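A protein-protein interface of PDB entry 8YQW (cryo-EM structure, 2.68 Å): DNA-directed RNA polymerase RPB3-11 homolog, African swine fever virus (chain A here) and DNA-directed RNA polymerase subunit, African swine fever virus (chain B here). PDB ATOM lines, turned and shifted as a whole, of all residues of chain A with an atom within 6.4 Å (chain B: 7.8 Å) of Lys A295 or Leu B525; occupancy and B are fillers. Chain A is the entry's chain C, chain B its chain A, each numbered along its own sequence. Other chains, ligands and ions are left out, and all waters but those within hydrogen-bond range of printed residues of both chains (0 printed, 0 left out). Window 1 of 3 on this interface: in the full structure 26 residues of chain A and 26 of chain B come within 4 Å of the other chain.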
ATOM      1  N   ARG A  52       0.440 -27.726 -16.571  1.00  0.00           N
ATOM      2  CA  ARG A  52      -0.487 -26.941 -17.375  1.00  0.00           C
ATOM      3  C   ARG A  52      -0.210 -25.449 -17.273  1.00  0.00           C
ATOM      4  O   ARG A  52      -0.448 -24.719 -18.241  1.00  0.00           O
ATOM      5  CB  ARG A  52      -1.925 -27.249 -16.945  1.00  0.00           C
ATOM      6  CG  ARG A  52      -2.981 -26.366 -17.576  1.00  0.00           C
ATOM      7  CD  ARG A  52      -4.382 -26.767 -17.147  1.00  0.00           C
ATOM      8  NE  ARG A  52      -4.510 -26.901 -15.701  1.00  0.00           N
ATOM      9  CZ  ARG A  52      -5.094 -27.925 -15.093  1.00  0.00           C
ATOM     10  NH1 ARG A  52      -5.659 -28.903 -15.778  1.00  0.00           N
ATOM     11  NH2 ARG A  52      -5.123 -27.960 -13.765  1.00  0.00           N
ATOM     12  N   ASP A 213      -4.505 -33.487 -12.683  1.00  0.00           N
ATOM     13  CA  ASP A 213      -3.230 -32.779 -12.803  1.00  0.00           C
ATOM     14  C   ASP A 213      -2.535 -33.240 -14.074  1.00  0.00           C
ATOM     15  O   ASP A 213      -1.584 -34.028 -14.032  1.00  0.00           O
ATOM     16  CB  ASP A 213      -2.348 -33.017 -11.576  1.00  0.00           C
ATOM     17  CG  ASP A 213      -1.177 -32.063 -11.511  1.00  0.00           C
ATOM     18  OD1 ASP A 213      -1.396 -30.877 -11.194  1.00  0.00           O
ATOM     19  OD2 ASP A 213      -0.038 -32.498 -11.779  1.00  0.00           O
ATOM     20  N   ILE A 290       2.255 -15.017 -14.984  1.00  0.00           N
ATOM     21  CA  ILE A 290       3.309 -15.115 -13.985  1.00  0.00           C
ATOM     22  C   ILE A 290       2.737 -15.533 -12.637  1.00  0.00           C
ATOM     23  O   ILE A 290       3.367 -16.289 -11.892  1.00  0.00           O
ATOM     24  CB  ILE A 290       4.075 -13.785 -13.895  1.00  0.00           C
ATOM     25  CG1 ILE A 290       4.725 -13.464 -15.239  1.00  0.00           C
ATOM     26  CG2 ILE A 290       5.140 -13.868 -12.842  1.00  0.00           C
ATOM     27  CD1 ILE A 290       5.605 -14.565 -15.767  1.00  0.00           C
ATOM     28  N   GLY A 291       1.541 -15.051 -12.299  1.00  0.00           N
ATOM     29  CA  GLY A 291       0.929 -15.449 -11.042  1.00  0.00           C
ATOM     30  C   GLY A 291       0.659 -16.939 -10.973  1.00  0.00           C
ATOM     31  O   GLY A 291       0.948 -17.592  -9.967  1.00  0.00           O
ATOM     32  N   ASN A 292       0.105 -17.498 -12.049  1.00  0.00           N
ATOM     33  CA  ASN A 292      -0.156 -18.931 -12.095  1.00  0.00           C
ATOM     34  C   ASN A 292       1.139 -19.729 -12.077  1.00  0.00           C
ATOM     35  O   ASN A 292       1.226 -20.757 -11.397  1.00  0.00           O
ATOM     36  CB  ASN A 292      -0.980 -19.275 -13.334  1.00  0.00           C
ATOM     37  CG  ASN A 292      -2.039 -20.317 -13.055  1.00  0.00           C
ATOM     38  OD1 ASN A 292      -2.765 -20.230 -12.069  1.00  0.00           O
ATOM     39  ND2 ASN A 292      -2.129 -21.317 -13.922  1.00  0.00           N
ATOM     40  N   LEU A 293       2.159 -19.274 -12.813  1.00  0.00           N
ATOM     41  CA  LEU A 293       3.450 -19.955 -12.775  1.00  0.00           C
ATOM     42  C   LEU A 293       4.023 -19.970 -11.364  1.00  0.00           C
ATOM     43  O   LEU A 293       4.475 -21.013 -10.873  1.00  0.00           O
ATOM     44  CB  LEU A 293       4.428 -19.286 -13.739  1.00  0.00           C
ATOM     45  CG  LEU A 293       4.469 -19.821 -15.166  1.00  0.00           C
ATOM     46  CD1 LEU A 293       5.284 -18.898 -16.050  1.00  0.00           C
ATOM     47  CD2 LEU A 293       5.047 -21.219 -15.172  1.00  0.00           C
ATOM     48  N   LEU A 294       4.008 -18.816 -10.697  1.00  0.00           N
ATOM     49  CA  LEU A 294       4.544 -18.717  -9.345  1.00  0.00           C
ATOM     50  C   LEU A 294       3.788 -19.627  -8.392  1.00  0.00           C
ATOM     51  O   LEU A 294       4.395 -20.380  -7.624  1.00  0.00           O
ATOM     52  CB  LEU A 294       4.481 -17.271  -8.862  1.00  0.00           C
ATOM     53  CG  LEU A 294       5.550 -16.302  -9.359  1.00  0.00           C
ATOM     54  CD1 LEU A 294       5.283 -14.919  -8.806  1.00  0.00           C
ATOM     55  CD2 LEU A 294       6.925 -16.786  -8.958  1.00  0.00           C
ATOM     56  N   LYS A 295       2.456 -19.571  -8.428  1.00  0.00           N
ATOM     57  CA  LYS A 295       1.662 -20.401  -7.531  1.00  0.00           C
ATOM     58  C   LYS A 295       1.942 -21.879  -7.767  1.00  0.00           C
ATOM     59  O   LYS A 295       2.188 -22.634  -6.820  1.00  0.00           O
ATOM     60  CB  LYS A 295       0.176 -20.095  -7.715  1.00  0.00           C
ATOM     61  CG  LYS A 295      -0.738 -20.886  -6.803  1.00  0.00           C
ATOM     62  CD  LYS A 295      -2.117 -20.268  -6.750  1.00  0.00           C
ATOM     63  CE  LYS A 295      -3.016 -20.820  -7.839  1.00  0.00           C
ATOM     64  NZ  LYS A 295      -3.634 -22.111  -7.443  1.00  0.00           N
ATOM     65  N   THR A 296       1.945 -22.304  -9.034  1.00  0.00           N
ATOM     66  CA  THR A 296       2.142 -23.714  -9.345  1.00  0.00           C
ATOM     67  C   THR A 296       3.514 -24.199  -8.898  1.00  0.00           C
ATOM     68  O   THR A 296       3.633 -25.268  -8.289  1.00  0.00           O
ATOM     69  CB  THR A 296       1.959 -23.947 -10.843  1.00  0.00           C
ATOM     70  OG1 THR A 296       0.617 -23.611 -11.215  1.00  0.00           O
ATOM     71  CG2 THR A 296       2.228 -25.397 -11.193  1.00  0.00           C
ATOM     72  N   TYR A 297       4.564 -23.423  -9.169  1.00  0.00           N
ATOM     73  CA  TYR A 297       5.901 -23.905  -8.848  1.00  0.00           C
ATOM     74  C   TYR A 297       6.218 -23.805  -7.362  1.00  0.00           C
ATOM     75  O   TYR A 297       6.938 -24.659  -6.835  1.00  0.00           O
ATOM     76  CB  TYR A 297       6.938 -23.161  -9.682  1.00  0.00           C
ATOM     77  CG  TYR A 297       7.137 -23.797 -11.036  1.00  0.00           C
ATOM     78  CD1 TYR A 297       6.254 -23.547 -12.074  1.00  0.00           C
ATOM     79  CD2 TYR A 297       8.193 -24.663 -11.269  1.00  0.00           C
ATOM     80  CE1 TYR A 297       6.425 -24.131 -13.309  1.00  0.00           C
ATOM     81  CE2 TYR A 297       8.371 -25.251 -12.504  1.00  0.00           C
ATOM     82  CZ  TYR A 297       7.484 -24.982 -13.519  1.00  0.00           C
ATOM     83  OH  TYR A 297       7.656 -25.565 -14.752  1.00  0.00           O
ATOM     84  N   ILE A 298       5.691 -22.795  -6.665  1.00  0.00           N
ATOM     85  CA  ILE A 298       5.820 -22.762  -5.212  1.00  0.00           C
ATOM     86  C   ILE A 298       5.100 -23.951  -4.597  1.00  0.00           C
ATOM     87  O   ILE A 298       5.614 -24.600  -3.678  1.00  0.00           O
ATOM     88  CB  ILE A 298       5.288 -21.428  -4.657  1.00  0.00           C
ATOM     89  CG1 ILE A 298       6.232 -20.281  -5.018  1.00  0.00           C
ATOM     90  CG2 ILE A 298       5.103 -21.505  -3.156  1.00  0.00           C
ATOM     91  CD1 ILE A 298       5.571 -18.924  -4.991  1.00  0.00           C
ATOM     92  N   TYR A 299       3.904 -24.263  -5.100  1.00  0.00           N
ATOM     93  CA  TYR A 299       3.143 -25.391  -4.579  1.00  0.00           C
ATOM     94  C   TYR A 299       3.857 -26.712  -4.835  1.00  0.00           C
ATOM     95  O   TYR A 299       3.840 -27.610  -3.987  1.00  0.00           O
ATOM     96  CB  TYR A 299       1.754 -25.385  -5.209  1.00  0.00           C
ATOM     97  CG  TYR A 299       0.856 -26.513  -4.786  1.00  0.00           C
ATOM     98  CD1 TYR A 299       0.563 -26.729  -3.451  1.00  0.00           C
ATOM     99  CD2 TYR A 299       0.281 -27.348  -5.727  1.00  0.00           C
ATOM    100  CE1 TYR A 299      -0.266 -27.753  -3.065  1.00  0.00           C
ATOM    101  CE2 TYR A 299      -0.548 -28.373  -5.351  1.00  0.00           C
ATOM    102  CZ  TYR A 299      -0.819 -28.570  -4.020  1.00  0.00           C
ATOM    103  OH  TYR A 299      -1.650 -29.590  -3.647  1.00  0.00           O
ATOM    104  N   GLU A 300       4.480 -26.857  -6.006  1.00  0.00           N
ATOM    105  CA  GLU A 300       5.261 -28.059  -6.282  1.00  0.00           C
ATOM    106  C   GLU A 300       6.492 -28.137  -5.390  1.00  0.00           C
ATOM    107  O   GLU A 300       6.890 -29.226  -4.964  1.00  0.00           O
ATOM    108  CB  GLU A 300       5.671 -28.096  -7.753  1.00  0.00           C
ATOM    109  CG  GLU A 300       4.537 -28.396  -8.713  1.00  0.00           C
ATOM    110  CD  GLU A 300       4.960 -28.264 -10.162  1.00  0.00           C
ATOM    111  OE1 GLU A 300       6.148 -27.976 -10.412  1.00  0.00           O
ATOM    112  OE2 GLU A 300       4.103 -28.446 -11.050  1.00  0.00           O
ATOM    113  N   VAL A 308      -1.101 -20.684  -0.587  1.00  0.00           N
ATOM    114  CA  VAL A 308      -0.523 -19.920  -1.688  1.00  0.00           C
ATOM    115  C   VAL A 308      -1.650 -19.508  -2.630  1.00  0.00           C
ATOM    116  O   VAL A 308      -2.517 -20.317  -2.971  1.00  0.00           O
ATOM    117  CB  VAL A 308       0.582 -20.712  -2.421  1.00  0.00           C
ATOM    118  CG1 VAL A 308       0.060 -22.037  -2.950  1.00  0.00           C
ATOM    119  CG2 VAL A 308       1.196 -19.879  -3.530  1.00  0.00           C
ATOM    120  N   GLY A 309      -1.653 -18.235  -3.018  1.00  0.00           N
ATOM    121  CA  GLY A 309      -2.667 -17.705  -3.916  1.00  0.00           C
ATOM    122  C   GLY A 309      -2.115 -16.514  -4.667  1.00  0.00           C
ATOM    123  O   GLY A 309      -1.112 -15.927  -4.262  1.00  0.00           O
ATOM    124  N   TYR A 310      -2.783 -16.145  -5.769  1.00  0.00           N
ATOM    125  CA  TYR A 310      -2.190 -15.178  -6.690  1.00  0.00           C
ATOM    126  C   TYR A 310      -3.174 -14.137  -7.221  1.00  0.00           C
ATOM    127  O   TYR A 310      -2.889 -13.509  -8.242  1.00  0.00           O
ATOM    128  CB  TYR A 310      -1.500 -15.909  -7.852  1.00  0.00           C
ATOM    129  CG  TYR A 310      -2.386 -16.294  -9.023  1.00  0.00           C
ATOM    130  CD1 TYR A 310      -3.062 -17.500  -9.034  1.00  0.00           C
ATOM    131  CD2 TYR A 310      -2.500 -15.477 -10.140  1.00  0.00           C
ATOM    132  CE1 TYR A 310      -3.856 -17.858 -10.098  1.00  0.00           C
ATOM    133  CE2 TYR A 310      -3.294 -15.823 -11.200  1.00  0.00           C
ATOM    134  CZ  TYR A 310      -3.967 -17.015 -11.180  1.00  0.00           C
ATOM    135  OH  TYR A 310      -4.756 -17.368 -12.249  1.00  0.00           O
ATOM    136  N   LEU A 321       0.517 -12.012  -4.774  1.00  0.00           N
ATOM    137  CA  LEU A 321       0.800 -13.400  -4.441  1.00  0.00           C
ATOM    138  C   LEU A 321       1.007 -13.508  -2.938  1.00  0.00           C
ATOM    139  O   LEU A 321       1.896 -12.856  -2.382  1.00  0.00           O
ATOM    140  CB  LEU A 321       2.033 -13.900  -5.193  1.00  0.00           C
ATOM    141  CG  LEU A 321       2.465 -15.355  -4.991  1.00  0.00           C
ATOM    142  CD1 LEU A 321       1.585 -16.298  -5.781  1.00  0.00           C
ATOM    143  CD2 LEU A 321       3.914 -15.535  -5.384  1.00  0.00           C
ATOM    144  N   MET B 522     -12.494 -31.849  -4.271  1.00  0.00           N
ATOM    145  CA  MET B 522     -11.421 -31.149  -4.957  1.00  0.00           C
ATOM    146  C   MET B 522     -10.130 -31.360  -4.185  1.00  0.00           C
ATOM    147  O   MET B 522     -10.147 -31.564  -2.970  1.00  0.00           O
ATOM    148  CB  MET B 522     -11.726 -29.654  -5.094  1.00  0.00           C
ATOM    149  CG  MET B 522     -11.804 -28.918  -3.775  1.00  0.00           C
ATOM    150  SD  MET B 522     -12.725 -27.375  -3.884  1.00  0.00           S
ATOM    151  CE  MET B 522     -14.401 -27.979  -3.738  1.00  0.00           C
ATOM    152  N   ASN B 523      -9.008 -31.314  -4.897  1.00  0.00           N
ATOM    153  CA  ASN B 523      -7.721 -31.539  -4.260  1.00  0.00           C
ATOM    154  C   ASN B 523      -7.302 -30.301  -3.470  1.00  0.00           C
ATOM    155  O   ASN B 523      -8.016 -29.299  -3.409  1.00  0.00           O
ATOM    156  CB  ASN B 523      -6.673 -31.935  -5.297  1.00  0.00           C
ATOM    157  CG  ASN B 523      -6.546 -30.929  -6.415  1.00  0.00           C
ATOM    158  OD1 ASN B 523      -7.208 -29.896  -6.414  1.00  0.00           O
ATOM    159  ND2 ASN B 523      -5.691 -31.228  -7.381  1.00  0.00           N
ATOM    160  N   LYS B 524      -6.125 -30.375  -2.845  1.00  0.00           N
ATOM    161  CA  LYS B 524      -5.670 -29.280  -1.994  1.00  0.00           C
ATOM    162  C   LYS B 524      -5.461 -27.999  -2.790  1.00  0.00           C
ATOM    163  O   LYS B 524      -5.809 -26.909  -2.326  1.00  0.00           O
ATOM    164  CB  LYS B 524      -4.383 -29.674  -1.271  1.00  0.00           C
ATOM    165  CG  LYS B 524      -3.721 -28.529  -0.531  1.00  0.00           C
ATOM    166  CD  LYS B 524      -2.409 -28.953   0.085  1.00  0.00           C
ATOM    167  CE  LYS B 524      -1.701 -27.781   0.727  1.00  0.00           C
ATOM    168  NZ  LYS B 524      -0.468 -28.213   1.427  1.00  0.00           N
ATOM    169  N   LEU B 525      -4.888 -28.111  -3.990  1.00  0.00           N
ATOM    170  CA  LEU B 525      -4.596 -26.921  -4.782  1.00  0.00           C
ATOM    171  C   LEU B 525      -5.866 -26.167  -5.148  1.00  0.00           C
ATOM    172  O   LEU B 525      -5.908 -24.934  -5.073  1.00  0.00           O
ATOM    173  CB  LEU B 525      -3.829 -27.309  -6.043  1.00  0.00           C
ATOM    174  CG  LEU B 525      -3.410 -26.160  -6.959  1.00  0.00           C
ATOM    175  CD1 LEU B 525      -2.531 -25.172  -6.213  1.00  0.00           C
ATOM    176  CD2 LEU B 525      -2.698 -26.699  -8.184  1.00  0.00           C
ATOM    177  N   HIS B 526      -6.911 -26.885  -5.555  1.00  0.00           N
ATOM    178  CA  HIS B 526      -8.147 -26.220  -5.938  1.00  0.00           C
ATOM    179  C   HIS B 526      -8.945 -25.757  -4.731  1.00  0.00           C
ATOM    180  O   HIS B 526      -9.660 -24.756  -4.819  1.00  0.00           O
ATOM    181  CB  HIS B 526      -8.984 -27.141  -6.821  1.00  0.00           C
ATOM    182  CG  HIS B 526      -8.424 -27.316  -8.196  1.00  0.00           C
ATOM    183  ND1 HIS B 526      -7.465 -28.258  -8.494  1.00  0.00           N
ATOM    184  CD2 HIS B 526      -8.675 -26.656  -9.351  1.00  0.00           C
ATOM    185  CE1 HIS B 526      -7.154 -28.176  -9.775  1.00  0.00           C
ATOM    186  NE2 HIS B 526      -7.875 -27.213 -10.317  1.00  0.00           N
ATOM    187  N   ALA B 527      -8.837 -26.460  -3.604  1.00  0.00           N
ATOM    188  CA  ALA B 527      -9.460 -25.980  -2.376  1.00  0.00           C
ATOM    189  C   ALA B 527      -8.832 -24.670  -1.922  1.00  0.00           C
ATOM    190  O   ALA B 527      -9.536 -23.766  -1.457  1.00  0.00           O
ATOM    191  CB  ALA B 527      -9.351 -27.039  -1.282  1.00  0.00           C
ATOM    192  N   MET B 528      -7.508 -24.552  -2.042  1.00  0.00           N
ATOM    193  CA  MET B 528      -6.840 -23.299  -1.708  1.00  0.00           C
ATOM    194  C   MET B 528      -7.260 -22.183  -2.652  1.00  0.00           C
ATOM    195  O   MET B 528      -7.286 -21.010  -2.266  1.00  0.00           O
ATOM    196  CB  MET B 528      -5.323 -23.486  -1.753  1.00  0.00           C
ATOM    197  CG  MET B 528      -4.723 -24.043  -0.484  1.00  0.00           C
ATOM    198  SD  MET B 528      -2.931 -23.910  -0.437  1.00  0.00           S
ATOM    199  CE  MET B 528      -2.491 -24.686  -1.984  1.00  0.00           C
ATOM    200  N   GLY B 529      -7.588 -22.527  -3.898  1.00  0.00           N
ATOM    201  CA  GLY B 529      -7.941 -21.523  -4.884  1.00  0.00           C
ATOM    202  C   GLY B 529      -9.289 -20.877  -4.656  1.00  0.00           C
ATOM    203  O   GLY B 529      -9.547 -19.802  -5.203  1.00  0.00           O
ATOM    204  N   LEU B 530     -10.157 -21.510  -3.871  1.00  0.00           N
ATOM    205  CA  LEU B 530     -11.444 -20.902  -3.564  1.00  0.00           C
ATOM    206  C   LEU B 530     -11.301 -19.732  -2.599  1.00  0.00           C
ATOM    207  O   LEU B 530     -12.139 -18.825  -2.600  1.00  0.00           O
ATOM    208  CB  LEU B 530     -12.396 -21.955  -2.999  1.00  0.00           C
ATOM    209  CG  LEU B 530     -13.307 -22.688  -3.986  1.00  0.00           C
ATOM    210  CD1 LEU B 530     -12.526 -23.559  -4.928  1.00  0.00           C
ATOM    211  CD2 LEU B 530     -14.322 -23.520  -3.234  1.00  0.00           C
ATOM    212  N   PHE B 531     -10.249 -19.725  -1.786  1.00  0.00           N
ATOM    213  CA  PHE B 531     -10.048 -18.691  -0.781  1.00  0.00           C
ATOM    214  C   PHE B 531      -9.112 -17.583  -1.231  1.00  0.00           C
ATOM    215  O   PHE B 531      -8.847 -16.665  -0.450  1.00  0.00           O
ATOM    216  CB  PHE B 531      -9.509 -19.312   0.506  1.00  0.00           C
ATOM    217  CG  PHE B 531     -10.515 -20.133   1.245  1.00  0.00           C
ATOM    218  CD1 PHE B 531     -11.441 -19.530   2.073  1.00  0.00           C
ATOM    219  CD2 PHE B 531     -10.536 -21.506   1.110  1.00  0.00           C
ATOM    220  CE1 PHE B 531     -12.368 -20.283   2.750  1.00  0.00           C
ATOM    221  CE2 PHE B 531     -11.460 -22.261   1.787  1.00  0.00           C
ATOM    222  CZ  PHE B 531     -12.376 -21.650   2.607  1.00  0.00           C
ATOM    223  N   GLN B 532      -8.608 -17.631  -2.458  1.00  0.00           N
ATOM    224  CA  GLN B 532      -7.610 -16.655  -2.868  1.00  0.00           C
ATOM    225  C   GLN B 532      -8.221 -15.345  -3.341  1.00  0.00           C
ATOM    226  O   GLN B 532      -7.476 -14.430  -3.699  1.00  0.00           O
ATOM    227  CB  GLN B 532      -6.707 -17.244  -3.954  1.00  0.00           C
ATOM    228  CG  GLN B 532      -7.365 -17.472  -5.293  1.00  0.00           C
ATOM    229  CD  GLN B 532      -6.467 -18.240  -6.240  1.00  0.00           C
ATOM    230  OE1 GLN B 532      -5.439 -18.776  -5.835  1.00  0.00           O
ATOM    231  NE2 GLN B 532      -6.848 -18.295  -7.507  1.00  0.00           N
ATOM    232  N   PHE B 541      -3.988 -24.966   5.291  1.00  0.00           N
ATOM    233  CA  PHE B 541      -4.052 -26.215   4.547  1.00  0.00           C
ATOM    234  C   PHE B 541      -2.807 -27.068   4.760  1.00  0.00           C
ATOM    235  O   PHE B 541      -2.525 -27.958   3.954  1.00  0.00           O
ATOM    236  CB  PHE B 541      -4.253 -25.935   3.057  1.00  0.00           C
ATOM    237  CG  PHE B 541      -5.595 -25.354   2.721  1.00  0.00           C
ATOM    238  CD1 PHE B 541      -5.826 -23.996   2.832  1.00  0.00           C
ATOM    239  CD2 PHE B 541      -6.624 -26.167   2.283  1.00  0.00           C
ATOM    240  CE1 PHE B 541      -7.056 -23.463   2.518  1.00  0.00           C
ATOM    241  CE2 PHE B 541      -7.856 -25.636   1.970  1.00  0.00           C
ATOM    242  CZ  PHE B 541      -8.072 -24.284   2.089  1.00  0.00           C
ATOM    243  N   TYR B 544      -2.591 -31.258   4.862  1.00  0.00           N
ATOM    244  CA  TYR B 544      -3.196 -31.793   3.652  1.00  0.00           C
ATOM    245  C   TYR B 544      -2.101 -32.107   2.647  1.00  0.00           C
ATOM    246  O   TYR B 544      -1.272 -31.245   2.344  1.00  0.00           O
ATOM    247  CB  TYR B 544      -4.195 -30.806   3.041  1.00  0.00           C
ATOM    248  CG  TYR B 544      -5.511 -30.712   3.773  1.00  0.00           C
ATOM    249  CD1 TYR B 544      -6.369 -31.796   3.837  1.00  0.00           C
ATOM    250  CD2 TYR B 544      -5.899 -29.534   4.390  1.00  0.00           C
ATOM    251  CE1 TYR B 544      -7.572 -31.712   4.501  1.00  0.00           C
ATOM    252  CE2 TYR B 544      -7.099 -29.439   5.054  1.00  0.00           C
ATOM    253  CZ  TYR B 544      -7.934 -30.531   5.109  1.00  0.00           C
ATOM    254  OH  TYR B 544      -9.134 -30.442   5.773  1.00  0.00           O
ATOM    255  N   SER B 545      -2.100 -33.334   2.142  1.00  0.00           N
ATOM    256  CA  SER B 545      -1.230 -33.690   1.040  1.00  0.00           C
ATOM    257  C   SER B 545      -1.772 -33.087  -0.253  1.00  0.00           C
ATOM    258  O   SER B 545      -2.947 -32.724  -0.334  1.00  0.00           O
ATOM    259  CB  SER B 545      -1.127 -35.210   0.927  1.00  0.00           C
ATOM    260  OG  SER B 545      -0.351 -35.610  -0.188  1.00  0.00           O
ATOM    261  N   PRO B 546      -0.927 -32.940  -1.275  1.00  0.00           N
ATOM    262  CA  PRO B 546      -1.441 -32.467  -2.570  1.00  0.00           C
ATOM    263  C   PRO B 546      -2.528 -33.348  -3.157  1.00  0.00           C
ATOM    264  O   PRO B 546      -3.368 -32.851  -3.917  1.00  0.00           O
ATOM    265  CB  PRO B 546      -0.187 -32.453  -3.451  1.00  0.00           C
ATOM    266  CG  PRO B 546       0.910 -32.167  -2.500  1.00  0.00           C
ATOM    267  CD  PRO B 546       0.543 -32.860  -1.213  1.00  0.00           C
ATOM    268  N   THR B 547      -2.542 -34.637  -2.833  1.00  0.00           N
ATOM    269  CA  THR B 547      -3.532 -35.558  -3.370  1.00  0.00           C
ATOM    270  C   THR B 547      -4.740 -35.738  -2.460  1.00  0.00           C
ATOM    271  O   THR B 547      -5.643 -36.507  -2.804  1.00  0.00           O
ATOM    272  CB  THR B 547      -2.889 -36.920  -3.637  1.00  0.00           C
ATOM    273  OG1 THR B 547      -2.362 -37.446  -2.415  1.00  0.00           O
ATOM    274  CG2 THR B 547      -1.765 -36.778  -4.645  1.00  0.00           C
ATOM    275  N   ASP B 548      -4.780 -35.065  -1.315  1.00  0.00           N
ATOM    276  CA  ASP B 548      -5.946 -35.146  -0.448  1.00  0.00           C
ATOM    277  C   ASP B 548      -7.126 -34.425  -1.082  1.00  0.00           C
ATOM    278  O   ASP B 548      -6.972 -33.398  -1.747  1.00  0.00           O
ATOM    279  CB  ASP B 548      -5.638 -34.551   0.923  1.00  0.00           C
ATOM    280  CG  ASP B 548      -4.729 -35.434   1.746  1.00  0.00           C
ATOM    281  OD1 ASP B 548      -4.635 -36.639   1.438  1.00  0.00           O
ATOM    282  OD2 ASP B 548      -4.110 -34.927   2.704  1.00  0.00           O
ATOM    283  N   LEU B 550     -10.898 -32.626  -0.722  1.00  0.00           N
ATOM    284  CA  LEU B 550     -11.790 -31.884   0.154  1.00  0.00           C
ATOM    285  C   LEU B 550     -13.100 -31.623  -0.571  1.00  0.00           C
ATOM    286  O   LEU B 550     -13.101 -31.252  -1.748  1.00  0.00           O
ATOM    287  CB  LEU B 550     -11.166 -30.552   0.583  1.00  0.00           C
ATOM    288  CG  LEU B 550      -9.922 -30.570   1.469  1.00  0.00           C
ATOM    289  CD1 LEU B 550      -8.665 -30.540   0.628  1.00  0.00           C
ATOM    290  CD2 LEU B 550      -9.950 -29.391   2.419  1.00  0.00           C
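The backbone NH (N) of Val A308 lies within hydrogen-bond range of the side-chain sulfur (SD) of Met B528 (3.7 Å).
The backbone carbonyl oxygen (O) of Phe B541 lies within hydrogen-bond range of the side-chain amino group (NZ) of Lys B524, at 3.3 Å.
O of Tyr B544 is in hydrogen-bond range of NZ of Lys B524, at 3.3 Å.
O of Asp B548 is in hydrogen-bond range of N of Lys B524 (3.3 Å).
The side-chain amide oxygen (OD1) of Asn A292 sits close to the side-chain hydroxyl (OH) of Tyr A310 (3.5 Å).
Among the printed residues, pairs that only touch across the chains: Lys A295 with Leu B525 (3.5 Å), Lys A295 with Gln B532 (3.8 Å), Tyr A299 with Lys B524 (3.6 Å), Tyr A299 with Leu B525 (3.5 Å), Tyr A299 with Met B528 (3.9 Å), Tyr A299 with Pro B546 (3.1 Å), Gly A309 with Gln B532 (3.5 Å) and Tyr A310 with Gln B532 (3.7 Å).
Leu B525 touches two residues of chain A.
Of the printed residues of chain B, Tyr A299 touches Lys B524, Leu B525, Met B528 and Pro B546.
Of the printed residues of chain B, Gly A309 touches Gln B532 (3.5 Å).
Of the printed residues of chain A, Met B528 touches Tyr A299 and Val A308.
Of the printed residues of chain A, Gln B532 touches Lys A295 (3.8 Å), Gly A309 (3.5 Å) and Tyr A310 (3.7 Å).
Printed residues of chain B within 4 Å of Val A308: Met B528 (3.7 Å).
Asp A213 touches none of the printed residues of chain B.
Leu B530 touches none of the printed residues of chain A.
The nearest residue of chain A that does not touch Leu B525 is Val A308 (5.2 Å).
Of the 17 printed residues of chain A, 5 touch a printed residue of chain B.
Printed residues of chain A that touch a printed residue of chain B: Lys A295, Tyr A299, Val A308, Gly A309 and Tyr A310.
Hydrophobic or aromatic side chains of chain A that line the printed part of chain B: Tyr A299, Val A308 and Tyr A310.
Along chain A the printed residues that touch a printed residue of chain B span positions 295 to 310.
Hydrophobic or aromatic side chains of chain B that line the printed part of chain A: Leu B525, Met B528 and Pro B546.
Among the printed residues, 9 pairs touch across the chains.
Among the printed residues, no Asp or Glu carboxylate lies within 4 Å of a Lys or Arg side-chain nitrogen of the other chain.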
